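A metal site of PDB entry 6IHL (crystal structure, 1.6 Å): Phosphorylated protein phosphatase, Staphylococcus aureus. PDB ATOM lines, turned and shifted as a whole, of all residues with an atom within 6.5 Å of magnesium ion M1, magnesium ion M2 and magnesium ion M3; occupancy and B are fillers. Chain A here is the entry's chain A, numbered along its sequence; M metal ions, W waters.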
ATOM      1  N   ARG A  14      10.712 -13.566 -13.905  1.00  0.00           N
ATOM      2  CA  ARG A  14      10.726 -13.675 -12.446  1.00  0.00           C
ATOM      3  C   ARG A  14       9.294 -13.857 -11.976  1.00  0.00           C
ATOM      4  O   ARG A  14       8.380 -13.184 -12.456  1.00  0.00           O
ATOM      5  CB  ARG A  14      11.353 -12.447 -11.786  1.00  0.00           C
ATOM      6  CG  ARG A  14      12.867 -12.535 -11.618  1.00  0.00           C
ATOM      7  CD  ARG A  14      13.286 -13.614 -10.631  1.00  0.00           C
ATOM      8  NE  ARG A  14      13.555 -13.040  -9.307  1.00  0.00           N
ATOM      9  CZ  ARG A  14      12.847 -13.308  -8.217  1.00  0.00           C
ATOM     10  NH1 ARG A  14      11.822 -14.150  -8.268  1.00  0.00           N
ATOM     11  NH2 ARG A  14      13.173 -12.726  -7.071  1.00  0.00           N
ATOM     12  N   GLU A  18      10.810  -9.477  -5.207  1.00  0.00           N
ATOM     13  CA  GLU A  18      11.398  -9.503  -3.877  1.00  0.00           C
ATOM     14  C   GLU A  18      12.214  -8.246  -3.573  1.00  0.00           C
ATOM     15  O   GLU A  18      12.853  -8.172  -2.525  1.00  0.00           O
ATOM     16  CB  GLU A  18      12.265 -10.758  -3.726  1.00  0.00           C
ATOM     17  CG  GLU A  18      11.408 -12.036  -3.806  1.00  0.00           C
ATOM     18  CD  GLU A  18      12.197 -13.313  -3.705  1.00  0.00           C
ATOM     19  OE1 GLU A  18      13.446 -13.245  -3.621  1.00  0.00           O
ATOM     20  OE2 GLU A  18      11.568 -14.381  -3.715  1.00  0.00           O
ATOM     21  N   ASP A  19      12.209  -7.275  -4.476  1.00  0.00           N
ATOM     22  CA  ASP A  19      12.741  -5.953  -4.169  1.00  0.00           C
ATOM     23  C   ASP A  19      11.722  -5.154  -3.372  1.00  0.00           C
ATOM     24  O   ASP A  19      10.505  -5.364  -3.490  1.00  0.00           O
ATOM     25  CB  ASP A  19      13.070  -5.175  -5.443  1.00  0.00           C
ATOM     26  CG  ASP A  19      14.349  -5.628  -6.143  1.00  0.00           C
ATOM     27  OD1 ASP A  19      15.072  -6.524  -5.682  1.00  0.00           O
ATOM     28  OD2 ASP A  19      14.649  -5.003  -7.179  1.00  0.00           O
ATOM     29  N   ASP A  37      17.012  -5.444  -1.708  1.00  0.00           N
ATOM     30  CA  ASP A  37      16.908  -6.552  -2.652  1.00  0.00           C
ATOM     31  C   ASP A  37      16.823  -7.845  -1.844  1.00  0.00           C
ATOM     32  O   ASP A  37      17.853  -8.356  -1.389  1.00  0.00           O
ATOM     33  CB  ASP A  37      18.105  -6.561  -3.615  1.00  0.00           C
ATOM     34  CG  ASP A  37      18.015  -7.668  -4.634  1.00  0.00           C
ATOM     35  OD1 ASP A  37      17.187  -8.603  -4.432  1.00  0.00           O
ATOM     36  OD2 ASP A  37      18.767  -7.627  -5.626  1.00  0.00           O
ATOM     37  N   GLY A  38      15.615  -8.382  -1.715  1.00  0.00           N
ATOM     38  CA  GLY A  38      15.432  -9.634  -1.008  1.00  0.00           C
ATOM     39  C   GLY A  38      16.063 -10.801  -1.745  1.00  0.00           C
ATOM     40  O   GLY A  38      16.081 -10.850  -2.986  1.00  0.00           O
ATOM     41  N   MET A  39      16.588 -11.765  -0.993  1.00  0.00           N
ATOM     42  CA  MET A  39      17.420 -12.813  -1.579  1.00  0.00           C
ATOM     43  C   MET A  39      16.548 -13.847  -2.275  1.00  0.00           C
ATOM     44  O   MET A  39      15.707 -14.497  -1.627  1.00  0.00           O
ATOM     45  CB  MET A  39      18.294 -13.482  -0.527  1.00  0.00           C
ATOM     46  CG  MET A  39      19.511 -12.674  -0.098  1.00  0.00           C
ATOM     47  SD  MET A  39      20.778 -13.793   0.560  1.00  0.00           S
ATOM     48  CE  MET A  39      19.913 -14.456   1.993  1.00  0.00           C
ATOM     49  N   GLY A  40      16.745 -14.011  -3.586  1.00  0.00           N
ATOM     50  CA  GLY A  40      16.025 -15.018  -4.327  1.00  0.00           C
ATOM     51  C   GLY A  40      16.553 -16.424  -4.141  1.00  0.00           C
ATOM     52  O   GLY A  40      15.807 -17.378  -4.339  1.00  0.00           O
ATOM     53  N   GLY A  41      17.821 -16.554  -3.749  1.00  0.00           N
ATOM     54  CA  GLY A  41      18.411 -17.856  -3.515  1.00  0.00           C
ATOM     55  C   GLY A  41      18.010 -18.517  -2.221  1.00  0.00           C
ATOM     56  O   GLY A  41      18.375 -19.668  -1.984  1.00  0.00           O
ATOM     57  N   ASP A 120      24.808  -5.894  -2.380  1.00  0.00           N
ATOM     58  CA  ASP A 120      25.225  -5.455  -3.715  1.00  0.00           C
ATOM     59  C   ASP A 120      24.186  -4.577  -4.393  1.00  0.00           C
ATOM     60  O   ASP A 120      24.266  -4.381  -5.616  1.00  0.00           O
ATOM     61  CB  ASP A 120      25.561  -6.664  -4.594  1.00  0.00           C
ATOM     62  CG  ASP A 120      24.340  -7.451  -5.014  1.00  0.00           C
ATOM     63  OD1 ASP A 120      23.257  -7.296  -4.402  1.00  0.00           O
ATOM     64  OD2 ASP A 120      24.451  -8.247  -5.962  1.00  0.00           O
ATOM     65  N   ASP A 137      30.178  -3.145  -3.713  1.00  0.00           N
ATOM     66  CA  ASP A 137      29.385  -4.360  -3.681  1.00  0.00           C
ATOM     67  C   ASP A 137      29.955  -5.373  -2.694  1.00  0.00           C
ATOM     68  O   ASP A 137      31.116  -5.775  -2.804  1.00  0.00           O
ATOM     69  CB  ASP A 137      29.351  -5.024  -5.064  1.00  0.00           C
ATOM     70  CG  ASP A 137      28.454  -4.334  -6.060  1.00  0.00           C
ATOM     71  OD1 ASP A 137      27.989  -3.193  -5.799  1.00  0.00           O
ATOM     72  OD2 ASP A 137      28.233  -4.927  -7.148  1.00  0.00           O
ATOM     73  N   SER A 139      29.799  -8.571  -2.729  1.00  0.00           N
ATOM     74  CA  SER A 139      29.511  -9.725  -3.564  1.00  0.00           C
ATOM     75  C   SER A 139      30.738 -10.606  -3.648  1.00  0.00           C
ATOM     76  O   SER A 139      31.873 -10.158  -3.497  1.00  0.00           O
ATOM     77  CB  SER A 139      29.062  -9.318  -4.974  1.00  0.00           C
ATOM     78  OG  SER A 139      30.124  -8.707  -5.691  1.00  0.00           O
ATOM     79  N   ARG A 161      28.148 -15.607  -9.683  1.00  0.00           N
ATOM     80  CA  ARG A 161      27.989 -14.184  -9.844  1.00  0.00           C
ATOM     81  C   ARG A 161      26.885 -13.529  -9.014  1.00  0.00           C
ATOM     82  O   ARG A 161      26.931 -12.343  -8.756  1.00  0.00           O
ATOM     83  CB  ARG A 161      27.868 -13.804 -11.337  1.00  0.00           C
ATOM     84  CG  ARG A 161      26.446 -13.749 -11.850  1.00  0.00           C
ATOM     85  CD  ARG A 161      26.266 -14.198 -13.289  1.00  0.00           C
ATOM     86  NE  ARG A 161      25.152 -15.132 -13.382  1.00  0.00           N
ATOM     87  CZ  ARG A 161      25.221 -16.302 -13.996  1.00  0.00           C
ATOM     88  NH1 ARG A 161      26.356 -16.633 -14.567  1.00  0.00           N
ATOM     89  NH2 ARG A 161      24.179 -17.122 -14.034  1.00  0.00           N
ATOM     90  N   ASN A 162      25.894 -14.292  -8.592  1.00  0.00           N
ATOM     91  CA  ASN A 162      24.837 -13.750  -7.833  1.00  0.00           C
ATOM     92  C   ASN A 162      25.041 -13.795  -6.324  1.00  0.00           C
ATOM     93  O   ASN A 162      24.279 -13.229  -5.589  1.00  0.00           O
ATOM     94  CB  ASN A 162      23.544 -14.451  -8.221  1.00  0.00           C
ATOM     95  CG  ASN A 162      23.087 -14.103  -9.609  1.00  0.00           C
ATOM     96  OD1 ASN A 162      23.282 -12.988 -10.064  1.00  0.00           O
ATOM     97  ND2 ASN A 162      22.512 -15.054 -10.305  1.00  0.00           N
ATOM     98  N   ILE A 163      26.121 -14.442  -5.891  1.00  0.00           N
ATOM     99  CA  ILE A 163      26.383 -14.602  -4.470  1.00  0.00           C
ATOM    100  C   ILE A 163      26.810 -13.347  -3.775  1.00  0.00           C
ATOM    101  O   ILE A 163      27.674 -12.662  -4.254  1.00  0.00           O
ATOM    102  CB  ILE A 163      27.455 -15.635  -4.231  1.00  0.00           C
ATOM    103  CG1 ILE A 163      26.979 -16.959  -4.752  1.00  0.00           C
ATOM    104  CG2 ILE A 163      27.758 -15.779  -2.760  1.00  0.00           C
ATOM    105  CD1 ILE A 163      27.834 -18.098  -4.291  1.00  0.00           C
ATOM    106  N   ILE A 164      26.196 -13.062  -2.634  1.00  0.00           N
ATOM    107  CA  ILE A 164      26.559 -11.873  -1.870  1.00  0.00           C
ATOM    108  C   ILE A 164      27.151 -12.292  -0.534  1.00  0.00           C
ATOM    109  O   ILE A 164      26.841 -13.359   0.011  1.00  0.00           O
ATOM    110  CB  ILE A 164      25.365 -10.907  -1.697  1.00  0.00           C
ATOM    111  CG1 ILE A 164      24.159 -11.624  -1.106  1.00  0.00           C
ATOM    112  CG2 ILE A 164      25.000 -10.277  -3.036  1.00  0.00           C
ATOM    113  CD1 ILE A 164      22.927 -10.713  -0.991  1.00  0.00           C
ATOM    114  N   SER A 193      18.733  -1.561  -7.181  1.00  0.00           N
ATOM    115  CA  SER A 193      19.063  -2.968  -7.040  1.00  0.00           C
ATOM    116  C   SER A 193      19.892  -3.432  -8.225  1.00  0.00           C
ATOM    117  O   SER A 193      19.935  -2.784  -9.287  1.00  0.00           O
ATOM    118  CB  SER A 193      17.794  -3.822  -6.904  1.00  0.00           C
ATOM    119  OG  SER A 193      17.076  -3.886  -8.123  1.00  0.00           O
ATOM    120  N   ASP A 194      20.550  -4.568  -8.049  1.00  0.00           N
ATOM    121  CA  ASP A 194      21.398  -5.106  -9.111  1.00  0.00           C
ATOM    122  C   ASP A 194      20.610  -5.515 -10.350  1.00  0.00           C
ATOM    123  O   ASP A 194      21.228  -5.762 -11.383  1.00  0.00           O
ATOM    124  CB  ASP A 194      22.241  -6.266  -8.561  1.00  0.00           C
ATOM    125  CG  ASP A 194      21.407  -7.484  -8.138  1.00  0.00           C
ATOM    126  OD1 ASP A 194      20.154  -7.413  -8.122  1.00  0.00           O
ATOM    127  OD2 ASP A 194      22.021  -8.529  -7.826  1.00  0.00           O
ATOM    128  N   GLY A 195      19.276  -5.589 -10.287  1.00  0.00           N
ATOM    129  CA  GLY A 195      18.517  -5.840 -11.491  1.00  0.00           C
ATOM    130  C   GLY A 195      18.703  -4.773 -12.559  1.00  0.00           C
ATOM    131  O   GLY A 195      18.518  -5.046 -13.745  1.00  0.00           O
ATOM    132  N   ASP A 198      23.306  -4.890 -13.203  1.00  0.00           N
ATOM    133  CA  ASP A 198      23.777  -6.146 -13.802  1.00  0.00           C
ATOM    134  C   ASP A 198      23.591  -6.152 -15.310  1.00  0.00           C
ATOM    135  O   ASP A 198      24.241  -6.950 -16.000  1.00  0.00           O
ATOM    136  CB  ASP A 198      23.026  -7.354 -13.228  1.00  0.00           C
ATOM    137  CG  ASP A 198      23.507  -7.744 -11.847  1.00  0.00           C
ATOM    138  OD1 ASP A 198      24.461  -7.115 -11.356  1.00  0.00           O
ATOM    139  OD2 ASP A 198      22.949  -8.719 -11.276  1.00  0.00           O
ATOM    140  N   ASP A 233      15.958 -10.183 -13.600  1.00  0.00           N
ATOM    141  CA  ASP A 233      15.819  -9.966 -12.169  1.00  0.00           C
ATOM    142  C   ASP A 233      14.780  -8.873 -11.936  1.00  0.00           C
ATOM    143  O   ASP A 233      14.411  -8.141 -12.852  1.00  0.00           O
ATOM    144  CB  ASP A 233      17.176  -9.576 -11.561  1.00  0.00           C
ATOM    145  CG  ASP A 233      17.193  -9.625 -10.041  1.00  0.00           C
ATOM    146  OD1 ASP A 233      16.224 -10.123  -9.412  1.00  0.00           O
ATOM    147  OD2 ASP A 233      18.214  -9.194  -9.463  1.00  0.00           O
ATOM    148  N   ASN A 234      14.301  -8.804 -10.686  1.00  0.00           N
ATOM    149  CA  ASN A 234      13.574  -7.622 -10.239  1.00  0.00           C
ATOM    150  C   ASN A 234      14.438  -6.380 -10.430  1.00  0.00           C
ATOM    151  O   ASN A 234      15.627  -6.402 -10.106  1.00  0.00           O
ATOM    152  CB  ASN A 234      13.184  -7.735  -8.769  1.00  0.00           C
ATOM    153  CG  ASN A 234      12.521  -9.058  -8.420  1.00  0.00           C
ATOM    154  OD1 ASN A 234      12.770  -9.622  -7.351  1.00  0.00           O
ATOM    155  ND2 ASN A 234      11.680  -9.569  -9.320  1.00  0.00           N
HETATM  156 MG    MG M   1      18.552  -8.588  -7.473  1.00  0.00          MG
HETATM  157 MG    MG M   2      16.425 -10.363  -4.968  1.00  0.00          MG
HETATM  158 MG    MG M   3      23.978  -9.340  -7.566  1.00  0.00          MG
HETATM  159  O   HOH W   1      24.967  -7.840  -8.785  1.00  0.00           O
HETATM  160  O   HOH W   2      25.917 -10.361  -7.310  1.00  0.00           O
HETATM  161  O   HOH W   3      14.775  -9.203  -5.423  1.00  0.00           O
HETATM  162  O   HOH W   4      15.342 -12.063  -5.537  1.00  0.00           O
HETATM  163  O   HOH W   5      23.750 -10.321  -9.398  1.00  0.00           O
HETATM  164  O   HOH W   6      17.226 -10.116  -6.952  1.00  0.00           O
HETATM  165  O   HOH W   7      17.028  -7.192  -7.736  1.00  0.00           O
HETATM  166  O   HOH W   8      23.094 -10.808  -6.448  1.00  0.00           O
HETATM  167  O   HOH W   9      20.006 -10.060  -7.098  1.00  0.00           O
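The backbone carbonyl oxygen of Glu 18 is in hydrogen-bond range of the backbone NH of Gly 38 (2.9 Å). N of Gly 40 lies close to OE1 of Glu 18, at 3.4 Å. NE of Arg 14 lies within salt-bridge range of OD1 of Asp 233, at 3.96 Å.
Within 4 Å of magnesium ion M1: Asp 37, Asp 194 and Asp 233.
Merely in contact with magnesium ion M2: Gly 40.
OD2 of Asp 198 touches magnesium ion M3, at 3.9 Å. The nearest printed residue that does not touch magnesium ion M3 is Asn 162 (4.4 Å).
Magnesium ion M1 is bound by water W7 (2.1 Å), water W6 (2.1 Å), OD1 of Asp 194 (2.1 Å), OD2 of Asp 37 (2.1 Å), water W9 (2.1 Å) and OD2 of Asp 233 (2.1 Å). Magnesium ion M1 has six donor atoms within binding distance.
Magnesium ion M2 is bound by OD1 of Asp 37 (2.0 Å). Magnesium ion M2 is bound by water W3, 2.1 Å away. O of Gly 38 is bound to magnesium ion M2. Magnesium ion M2 is bound by water W4, 2.1 Å away. Magnesium ion M2 is bound by water W6 (2.2 Å). Magnesium ion M2 has five donor atoms within binding distance.
Magnesium ion M3 is bound by OD2 of Asp 120 (2.0 Å). Magnesium ion M3 is bound by water W8 (2.0 Å). Magnesium ion M3 is bound by water W5 (2.1 Å). Magnesium ion M3 is bound by OD2 of Asp 194, 2.1 Å away. Water W1 binds magnesium ion M3 (2.2 Å). Water W2 is bound to magnesium ion M3 (2.2 Å).
Water W3 bridges the side-chain carboxylate of Asp 19 and the side-chain amide oxygen of Asn 234. Water W4 lies within hydrogen-bond range of NH2 of Arg 14 (2.7 Å), OE1 of Glu 18 (2.9 Å) and N of Gly 40 (3.1 Å). Water W5 bridges the side-chain carboxylate (OD2) of Asp 198 (2.6 Å) and the side-chain amide oxygen (OD1) of Asn 162 (2.8 Å).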
